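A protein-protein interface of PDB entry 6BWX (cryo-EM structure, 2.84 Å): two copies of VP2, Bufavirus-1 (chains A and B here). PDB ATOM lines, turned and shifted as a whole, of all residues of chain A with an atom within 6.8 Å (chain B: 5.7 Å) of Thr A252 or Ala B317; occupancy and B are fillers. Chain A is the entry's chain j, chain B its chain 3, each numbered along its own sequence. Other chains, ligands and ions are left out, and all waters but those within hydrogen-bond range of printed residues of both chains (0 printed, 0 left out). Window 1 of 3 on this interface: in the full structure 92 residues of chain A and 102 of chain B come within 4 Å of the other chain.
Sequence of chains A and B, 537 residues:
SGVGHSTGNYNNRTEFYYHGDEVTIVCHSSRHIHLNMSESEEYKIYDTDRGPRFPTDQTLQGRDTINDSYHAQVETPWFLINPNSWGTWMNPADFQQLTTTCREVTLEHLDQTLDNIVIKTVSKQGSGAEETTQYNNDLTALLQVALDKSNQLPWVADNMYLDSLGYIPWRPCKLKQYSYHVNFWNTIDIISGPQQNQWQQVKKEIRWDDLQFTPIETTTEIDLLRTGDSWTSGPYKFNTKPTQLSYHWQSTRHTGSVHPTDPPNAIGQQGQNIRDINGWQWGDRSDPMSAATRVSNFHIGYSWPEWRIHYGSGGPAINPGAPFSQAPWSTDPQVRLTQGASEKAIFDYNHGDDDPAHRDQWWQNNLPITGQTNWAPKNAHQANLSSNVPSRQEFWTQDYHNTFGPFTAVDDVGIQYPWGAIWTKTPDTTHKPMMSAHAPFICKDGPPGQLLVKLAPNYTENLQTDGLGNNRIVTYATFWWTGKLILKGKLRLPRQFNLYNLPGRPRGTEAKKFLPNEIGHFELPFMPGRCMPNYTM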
ATOM      1  N   GLN A 250      32.903 -23.054 -17.240  1.00  0.00           N
ATOM      2  CA  GLN A 250      31.931 -22.569 -18.206  1.00  0.00           C
ATOM      3  C   GLN A 250      31.035 -23.694 -18.693  1.00  0.00           C
ATOM      4  O   GLN A 250      31.520 -24.750 -19.103  1.00  0.00           O
ATOM      5  CB  GLN A 250      32.629 -21.934 -19.404  1.00  0.00           C
ATOM      6  CG  GLN A 250      33.316 -20.635 -19.133  1.00  0.00           C
ATOM      7  CD  GLN A 250      33.987 -20.085 -20.355  1.00  0.00           C
ATOM      8  OE1 GLN A 250      34.370 -20.828 -21.244  1.00  0.00           O
ATOM      9  NE2 GLN A 250      34.119 -18.774 -20.420  1.00  0.00           N
ATOM     10  N   SER A 251      29.730 -23.463 -18.654  1.00  0.00           N
ATOM     11  CA  SER A 251      28.788 -24.293 -19.377  1.00  0.00           C
ATOM     12  C   SER A 251      28.570 -23.681 -20.750  1.00  0.00           C
ATOM     13  O   SER A 251      29.278 -22.762 -21.161  1.00  0.00           O
ATOM     14  CB  SER A 251      27.473 -24.422 -18.622  1.00  0.00           C
ATOM     15  OG  SER A 251      26.815 -23.181 -18.540  1.00  0.00           O
ATOM     16  N   THR A 252      27.591 -24.185 -21.481  1.00  0.00           N
ATOM     17  CA  THR A 252      27.238 -23.551 -22.737  1.00  0.00           C
ATOM     18  C   THR A 252      26.451 -22.266 -22.535  1.00  0.00           C
ATOM     19  O   THR A 252      26.290 -21.503 -23.492  1.00  0.00           O
ATOM     20  CB  THR A 252      26.462 -24.537 -23.605  1.00  0.00           C
ATOM     21  OG1 THR A 252      26.163 -23.939 -24.869  1.00  0.00           O
ATOM     22  CG2 THR A 252      25.198 -24.944 -22.923  1.00  0.00           C
ATOM     23  N   ARG A 253      25.963 -22.004 -21.324  1.00  0.00           N
ATOM     24  CA  ARG A 253      25.397 -20.703 -20.997  1.00  0.00           C
ATOM     25  C   ARG A 253      26.449 -19.675 -20.619  1.00  0.00           C
ATOM     26  O   ARG A 253      26.159 -18.480 -20.652  1.00  0.00           O
ATOM     27  CB  ARG A 253      24.387 -20.833 -19.863  1.00  0.00           C
ATOM     28  CG  ARG A 253      23.098 -21.488 -20.265  1.00  0.00           C
ATOM     29  CD  ARG A 253      22.310 -20.569 -21.162  1.00  0.00           C
ATOM     30  NE  ARG A 253      21.933 -19.353 -20.458  1.00  0.00           N
ATOM     31  CZ  ARG A 253      20.844 -19.234 -19.714  1.00  0.00           C
ATOM     32  NH1 ARG A 253      20.013 -20.252 -19.592  1.00  0.00           N
ATOM     33  NH2 ARG A 253      20.574 -18.096 -19.100  1.00  0.00           N
ATOM     34  N   HIS A 254      27.644 -20.104 -20.237  1.00  0.00           N
ATOM     35  CA  HIS A 254      28.728 -19.182 -19.940  1.00  0.00           C
ATOM     36  C   HIS A 254      29.619 -18.908 -21.137  1.00  0.00           C
ATOM     37  O   HIS A 254      30.459 -18.008 -21.070  1.00  0.00           O
ATOM     38  CB  HIS A 254      29.606 -19.740 -18.823  1.00  0.00           C
ATOM     39  CG  HIS A 254      28.869 -20.060 -17.564  1.00  0.00           C
ATOM     40  ND1 HIS A 254      28.416 -19.095 -16.697  1.00  0.00           N
ATOM     41  CD2 HIS A 254      28.509 -21.246 -17.026  1.00  0.00           C
ATOM     42  CE1 HIS A 254      27.810 -19.673 -15.677  1.00  0.00           C
ATOM     43  NE2 HIS A 254      27.849 -20.977 -15.855  1.00  0.00           N
ATOM     44  N   THR A 255      29.480 -19.676 -22.213  1.00  0.00           N
ATOM     45  CA  THR A 255      30.543 -19.743 -23.207  1.00  0.00           C
ATOM     46  C   THR A 255      30.505 -18.595 -24.206  1.00  0.00           C
ATOM     47  O   THR A 255      31.529 -17.952 -24.461  1.00  0.00           O
ATOM     48  CB  THR A 255      30.475 -21.078 -23.940  1.00  0.00           C
ATOM     49  OG1 THR A 255      30.654 -22.140 -23.000  1.00  0.00           O
ATOM     50  CG2 THR A 255      31.571 -21.160 -24.976  1.00  0.00           C
ATOM     51  N   GLY A 256      29.353 -18.319 -24.782  1.00  0.00           N
ATOM     52  CA  GLY A 256      29.309 -17.586 -26.029  1.00  0.00           C
ATOM     53  C   GLY A 256      29.264 -16.086 -25.869  1.00  0.00           C
ATOM     54  O   GLY A 256      29.788 -15.509 -24.915  1.00  0.00           O
ATOM     55  N   ALA A 291      18.594 -16.154 -23.866  1.00  0.00           N
ATOM     56  CA  ALA A 291      19.912 -16.766 -23.904  1.00  0.00           C
ATOM     57  C   ALA A 291      19.826 -18.279 -23.822  1.00  0.00           C
ATOM     58  O   ALA A 291      20.766 -18.976 -24.216  1.00  0.00           O
ATOM     59  CB  ALA A 291      20.777 -16.223 -22.772  1.00  0.00           C
ATOM     60  N   ALA A 292      18.716 -18.807 -23.316  1.00  0.00           N
ATOM     61  CA  ALA A 292      18.556 -20.253 -23.265  1.00  0.00           C
ATOM     62  C   ALA A 292      18.454 -20.843 -24.661  1.00  0.00           C
ATOM     63  O   ALA A 292      19.044 -21.890 -24.943  1.00  0.00           O
ATOM     64  CB  ALA A 292      17.325 -20.614 -22.444  1.00  0.00           C
ATOM     65  N   THR A 293      17.712 -20.189 -25.546  1.00  0.00           N
ATOM     66  CA  THR A 293      17.490 -20.681 -26.894  1.00  0.00           C
ATOM     67  C   THR A 293      18.468 -20.107 -27.905  1.00  0.00           C
ATOM     68  O   THR A 293      18.287 -20.319 -29.104  1.00  0.00           O
ATOM     69  CB  THR A 293      16.060 -20.389 -27.330  1.00  0.00           C
ATOM     70  OG1 THR A 293      15.828 -18.981 -27.286  1.00  0.00           O
ATOM     71  CG2 THR A 293      15.088 -21.078 -26.404  1.00  0.00           C
ATOM     72  N   ARG A 294      19.470 -19.359 -27.463  1.00  0.00           N
ATOM     73  CA  ARG A 294      20.518 -18.926 -28.372  1.00  0.00           C
ATOM     74  C   ARG A 294      21.202 -20.131 -28.991  1.00  0.00           C
ATOM     75  O   ARG A 294      21.591 -21.065 -28.287  1.00  0.00           O
ATOM     76  CB  ARG A 294      21.555 -18.082 -27.640  1.00  0.00           C
ATOM     77  CG  ARG A 294      22.681 -17.627 -28.537  1.00  0.00           C
ATOM     78  CD  ARG A 294      23.704 -16.804 -27.800  1.00  0.00           C
ATOM     79  NE  ARG A 294      24.461 -17.588 -26.834  1.00  0.00           N
ATOM     80  CZ  ARG A 294      25.546 -18.290 -27.135  1.00  0.00           C
ATOM     81  NH1 ARG A 294      26.179 -18.973 -26.199  1.00  0.00           N
ATOM     82  NH2 ARG A 294      25.995 -18.309 -28.375  1.00  0.00           N
ATOM     83  N   SER A 296      24.250 -22.119 -30.374  1.00  0.00           N
ATOM     84  CA  SER A 296      25.676 -22.154 -30.119  1.00  0.00           C
ATOM     85  C   SER A 296      26.299 -23.225 -30.999  1.00  0.00           C
ATOM     86  O   SER A 296      25.613 -24.103 -31.520  1.00  0.00           O
ATOM     87  CB  SER A 296      25.966 -22.428 -28.646  1.00  0.00           C
ATOM     88  OG  SER A 296      25.453 -23.686 -28.261  1.00  0.00           O
ATOM     89  N   ASN A 297      27.612 -23.139 -31.170  1.00  0.00           N
ATOM     90  CA  ASN A 297      28.292 -24.065 -32.062  1.00  0.00           C
ATOM     91  C   ASN A 297      28.495 -25.422 -31.415  1.00  0.00           C
ATOM     92  O   ASN A 297      28.495 -26.441 -32.110  1.00  0.00           O
ATOM     93  CB  ASN A 297      29.635 -23.485 -32.474  1.00  0.00           C
ATOM     94  CG  ASN A 297      29.489 -22.216 -33.245  1.00  0.00           C
ATOM     95  OD1 ASN A 297      28.475 -21.989 -33.886  1.00  0.00           O
ATOM     96  ND2 ASN A 297      30.479 -21.350 -33.151  1.00  0.00           N
ATOM     97  N   PHE A 298      28.662 -25.458 -30.101  1.00  0.00           N
ATOM     98  CA  PHE A 298      28.982 -26.684 -29.399  1.00  0.00           C
ATOM     99  C   PHE A 298      28.106 -26.770 -28.167  1.00  0.00           C
ATOM    100  O   PHE A 298      27.385 -25.835 -27.825  1.00  0.00           O
ATOM    101  CB  PHE A 298      30.453 -26.732 -29.011  1.00  0.00           C
ATOM    102  CG  PHE A 298      31.377 -26.457 -30.147  1.00  0.00           C
ATOM    103  CD1 PHE A 298      31.560 -27.384 -31.145  1.00  0.00           C
ATOM    104  CD2 PHE A 298      32.096 -25.283 -30.197  1.00  0.00           C
ATOM    105  CE1 PHE A 298      32.418 -27.134 -32.185  1.00  0.00           C
ATOM    106  CE2 PHE A 298      32.960 -25.032 -31.233  1.00  0.00           C
ATOM    107  CZ  PHE A 298      33.120 -25.958 -32.225  1.00  0.00           C
ATOM    108  N   HIS A 299      28.141 -27.920 -27.513  1.00  0.00           N
ATOM    109  CA  HIS A 299      27.504 -28.058 -26.217  1.00  0.00           C
ATOM    110  C   HIS A 299      28.494 -28.692 -25.260  1.00  0.00           C
ATOM    111  O   HIS A 299      29.329 -29.501 -25.660  1.00  0.00           O
ATOM    112  CB  HIS A 299      26.239 -28.879 -26.298  1.00  0.00           C
ATOM    113  CG  HIS A 299      25.369 -28.747 -25.095  1.00  0.00           C
ATOM    114  ND1 HIS A 299      25.564 -29.481 -23.949  1.00  0.00           N
ATOM    115  CD2 HIS A 299      24.308 -27.947 -24.854  1.00  0.00           C
ATOM    116  CE1 HIS A 299      24.650 -29.149 -23.057  1.00  0.00           C
ATOM    117  NE2 HIS A 299      23.876 -28.219 -23.581  1.00  0.00           N
ATOM    118  N   ILE A 300      28.412 -28.304 -23.994  1.00  0.00           N
ATOM    119  CA  ILE A 300      29.391 -28.699 -22.991  1.00  0.00           C
ATOM    120  C   ILE A 300      28.729 -29.657 -22.017  1.00  0.00           C
ATOM    121  O   ILE A 300      27.757 -29.299 -21.343  1.00  0.00           O
ATOM    122  CB  ILE A 300      29.972 -27.480 -22.267  1.00  0.00           C
ATOM    123  CG1 ILE A 300      30.814 -26.663 -23.238  1.00  0.00           C
ATOM    124  CG2 ILE A 300      30.813 -27.911 -21.106  1.00  0.00           C
ATOM    125  CD1 ILE A 300      31.266 -25.359 -22.689  1.00  0.00           C
ATOM    126  N   GLY A 371      29.689 -26.429 -15.035  1.00  0.00           N
ATOM    127  CA  GLY A 371      29.469 -26.128 -16.422  1.00  0.00           C
ATOM    128  C   GLY A 371      29.511 -27.334 -17.320  1.00  0.00           C
ATOM    129  O   GLY A 371      28.985 -27.284 -18.435  1.00  0.00           O
ATOM    130  N   GLN A 372      30.112 -28.416 -16.862  1.00  0.00           N
ATOM    131  CA  GLN A 372      29.948 -29.721 -17.463  1.00  0.00           C
ATOM    132  C   GLN A 372      28.823 -30.492 -16.795  1.00  0.00           C
ATOM    133  O   GLN A 372      28.496 -31.599 -17.229  1.00  0.00           O
ATOM    134  CB  GLN A 372      31.268 -30.485 -17.358  1.00  0.00           C
ATOM    135  CG  GLN A 372      31.361 -31.750 -18.148  1.00  0.00           C
ATOM    136  CD  GLN A 372      32.733 -32.352 -18.066  1.00  0.00           C
ATOM    137  OE1 GLN A 372      33.633 -31.779 -17.467  1.00  0.00           O
ATOM    138  NE2 GLN A 372      32.905 -33.513 -18.669  1.00  0.00           N
ATOM    139  N   ALA A 380      14.987 -31.873 -19.921  1.00  0.00           N
ATOM    140  CA  ALA A 380      13.680 -32.022 -20.546  1.00  0.00           C
ATOM    141  C   ALA A 380      13.847 -31.924 -22.054  1.00  0.00           C
ATOM    142  O   ALA A 380      14.893 -31.501 -22.547  1.00  0.00           O
ATOM    143  CB  ALA A 380      12.692 -30.971 -20.040  1.00  0.00           C
ATOM    144  N   ARG B 308      16.173 -31.087 -26.831  1.00  0.00           N
ATOM    145  CA  ARG B 308      16.637 -31.368 -25.483  1.00  0.00           C
ATOM    146  C   ARG B 308      16.974 -30.069 -24.772  1.00  0.00           C
ATOM    147  O   ARG B 308      17.754 -29.261 -25.277  1.00  0.00           O
ATOM    148  CB  ARG B 308      17.886 -32.239 -25.549  1.00  0.00           C
ATOM    149  CG  ARG B 308      18.442 -32.700 -24.224  1.00  0.00           C
ATOM    150  CD  ARG B 308      17.530 -33.722 -23.604  1.00  0.00           C
ATOM    151  NE  ARG B 308      18.101 -34.322 -22.407  1.00  0.00           N
ATOM    152  CZ  ARG B 308      17.458 -35.195 -21.644  1.00  0.00           C
ATOM    153  NH1 ARG B 308      18.047 -35.704 -20.575  1.00  0.00           N
ATOM    154  NH2 ARG B 308      16.240 -35.593 -21.973  1.00  0.00           N
ATOM    155  N   ILE B 309      16.408 -29.866 -23.588  1.00  0.00           N
ATOM    156  CA  ILE B 309      16.756 -28.718 -22.760  1.00  0.00           C
ATOM    157  C   ILE B 309      17.710 -29.205 -21.682  1.00  0.00           C
ATOM    158  O   ILE B 309      17.430 -30.189 -20.991  1.00  0.00           O
ATOM    159  CB  ILE B 309      15.523 -28.041 -22.152  1.00  0.00           C
ATOM    160  CG1 ILE B 309      14.606 -27.527 -23.249  1.00  0.00           C
ATOM    161  CG2 ILE B 309      15.945 -26.860 -21.329  1.00  0.00           C
ATOM    162  CD1 ILE B 309      13.422 -28.399 -23.501  1.00  0.00           C
ATOM    163  N   HIS B 310      18.921 -28.673 -21.693  1.00  0.00           N
ATOM    164  CA  HIS B 310      19.970 -29.089 -20.763  1.00  0.00           C
ATOM    165  C   HIS B 310      19.871 -28.807 -19.260  1.00  0.00           C
ATOM    166  O   HIS B 310      20.266 -29.643 -18.455  1.00  0.00           O
ATOM    167  CB  HIS B 310      21.346 -28.682 -21.288  1.00  0.00           C
ATOM    168  CG  HIS B 310      22.475 -29.121 -20.412  1.00  0.00           C
ATOM    169  ND1 HIS B 310      22.311 -30.021 -19.384  1.00  0.00           N
ATOM    170  CD2 HIS B 310      23.789 -28.800 -20.423  1.00  0.00           C
ATOM    171  CE1 HIS B 310      23.469 -30.226 -18.790  1.00  0.00           C
ATOM    172  NE2 HIS B 310      24.383 -29.497 -19.402  1.00  0.00           N
ATOM    173  N   TYR B 311      19.378 -27.641 -18.877  1.00  0.00           N
ATOM    174  CA  TYR B 311      19.324 -27.262 -17.459  1.00  0.00           C
ATOM    175  C   TYR B 311      20.633 -27.557 -16.735  1.00  0.00           C
ATOM    176  O   TYR B 311      20.656 -28.232 -15.708  1.00  0.00           O
ATOM    177  CB  TYR B 311      18.158 -27.923 -16.729  1.00  0.00           C
ATOM    178  CG  TYR B 311      16.805 -27.352 -17.062  1.00  0.00           C
ATOM    179  CD1 TYR B 311      16.349 -26.205 -16.438  1.00  0.00           C
ATOM    180  CD2 TYR B 311      15.972 -27.974 -17.968  1.00  0.00           C
ATOM    181  CE1 TYR B 311      15.113 -25.682 -16.730  1.00  0.00           C
ATOM    182  CE2 TYR B 311      14.733 -27.459 -18.259  1.00  0.00           C
ATOM    183  CZ  TYR B 311      14.311 -26.311 -17.643  1.00  0.00           C
ATOM    184  OH  TYR B 311      13.075 -25.791 -17.933  1.00  0.00           O
ATOM    185  N   GLY B 312      21.734 -27.048 -17.268  1.00  0.00           N
ATOM    186  CA  GLY B 312      23.008 -27.168 -16.599  1.00  0.00           C
ATOM    187  C   GLY B 312      23.246 -26.032 -15.635  1.00  0.00           C
ATOM    188  O   GLY B 312      22.386 -25.193 -15.381  1.00  0.00           O
ATOM    189  N   GLY B 315      22.241 -22.223 -16.465  1.00  0.00           N
ATOM    190  CA  GLY B 315      20.868 -22.021 -16.839  1.00  0.00           C
ATOM    191  C   GLY B 315      20.349 -23.157 -17.676  1.00  0.00           C
ATOM    192  O   GLY B 315      21.081 -24.085 -18.020  1.00  0.00           O
ATOM    193  N   PRO B 316      19.072 -23.108 -18.033  1.00  0.00           N
ATOM    194  CA  PRO B 316      18.579 -24.018 -19.063  1.00  0.00           C
ATOM    195  C   PRO B 316      19.204 -23.666 -20.399  1.00  0.00           C
ATOM    196  O   PRO B 316      19.246 -22.502 -20.795  1.00  0.00           O
ATOM    197  CB  PRO B 316      17.070 -23.778 -19.059  1.00  0.00           C
ATOM    198  CG  PRO B 316      16.923 -22.412 -18.547  1.00  0.00           C
ATOM    199  CD  PRO B 316      18.005 -22.232 -17.530  1.00  0.00           C
ATOM    200  N   ALA B 317      19.719 -24.677 -21.077  1.00  0.00           N
ATOM    201  CA  ALA B 317      20.256 -24.517 -22.413  1.00  0.00           C
ATOM    202  C   ALA B 317      19.590 -25.548 -23.298  1.00  0.00           C
ATOM    203  O   ALA B 317      18.671 -26.249 -22.880  1.00  0.00           O
ATOM    204  CB  ALA B 317      21.771 -24.671 -22.439  1.00  0.00           C
ATOM    205  N   ILE B 318      20.051 -25.647 -24.531  1.00  0.00           N
ATOM    206  CA  ILE B 318      19.432 -26.533 -25.499  1.00  0.00           C
ATOM    207  C   ILE B 318      20.519 -27.249 -26.281  1.00  0.00           C
ATOM    208  O   ILE B 318      21.518 -26.642 -26.679  1.00  0.00           O
ATOM    209  CB  ILE B 318      18.473 -25.750 -26.413  1.00  0.00           C
ATOM    210  CG1 ILE B 318      17.779 -26.672 -27.402  1.00  0.00           C
ATOM    211  CG2 ILE B 318      19.197 -24.627 -27.082  1.00  0.00           C
ATOM    212  CD1 ILE B 318      16.581 -26.033 -28.038  1.00  0.00           C
ATOM    213  N   ASN B 319      20.335 -28.551 -26.467  1.00  0.00           N
ATOM    214  CA  ASN B 319      21.363 -29.418 -27.011  1.00  0.00           C
ATOM    215  C   ASN B 319      20.930 -29.851 -28.403  1.00  0.00           C
ATOM    216  O   ASN B 319      19.932 -30.571 -28.538  1.00  0.00           O
ATOM    217  CB  ASN B 319      21.559 -30.613 -26.092  1.00  0.00           C
ATOM    218  CG  ASN B 319      22.865 -31.316 -26.319  1.00  0.00           C
ATOM    219  OD1 ASN B 319      23.482 -31.187 -27.368  1.00  0.00           O
ATOM    220  ND2 ASN B 319      23.306 -32.057 -25.319  1.00  0.00           N
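Thr A252 touches Ala B317. Gly B315 touches Arg A253. CB of Ala A292 touches O of Pro B316 (3.2 Å). Ala A292 touches Ala B317. Ala A292 touches Ile B318 (O to CG2, 3.5 Å). His B310 touches His A299 (CD2 to CE1, 2.8 Å). O of Ile B318 touches CD2 of His A299, 3.6 Å away. ND1 of His A299 touches ND2 of Asn B319, at 3.7 Å. Ile A300 touches His B310 (O to NE2, 3.9 Å). Ala A380 touches Arg B308.
Thr A252 touches just one residue of chain B: Ala B317. Ala B317 touches just these residues of chain A: Thr A252 (3.5 Å) and Ala A292 (3.8 Å). Printed residues of chain B within 4 Å of Ala A292: Pro B316, Ala B317 and Ile B318. Of the printed residues of chain A, Asn B319 touches His A299. Gln A372 touches none of the printed residues of chain B. Gly A256 touches none of the printed residues of chain B.
No position is printed for both chains.
Printed residues of chain A that touch a printed residue of chain B: Thr A252, Arg A253, Ala A292, His A299, Ile A300 and Ala A380. Hydrophobic or aromatic side chains of chain A within 4 Å of the printed part of chain B: Ala A292 and His A299. Of the 10 printed residues of chain B, 8 touch a printed residue of chain A. Hydrophobic or aromatic side chains of chain B within 4 Å of the printed part of chain A: Ile B309, His B310, Pro B316, Ala B317 and Ile B318.
OG of Ser A296 lies within hydrogen-bond range of OG1 of Thr A252 (3.5 Å). N of Arg A253 is in hydrogen-bond range of OG of Ser A251 (3.1 Å). The backbone NH (N) of His B310 lies within hydrogen-bond range of the backbone carbonyl oxygen (O) of Ala B317, 2.7 Å away. The backbone carbonyl oxygen (O) of Arg B308 sits at hydrogen-bond distance from the backbone NH (N) of Asn B319 (2.9 Å).
The backbone NH (N) of Ile B309 lies within hydrogen-bond range of the backbone carbonyl oxygen (O) of Ala A380, 2.5 Å away. NH1 of Arg A253 lies within hydrogen-bond range of O of Pro B316, 2.7 Å away.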
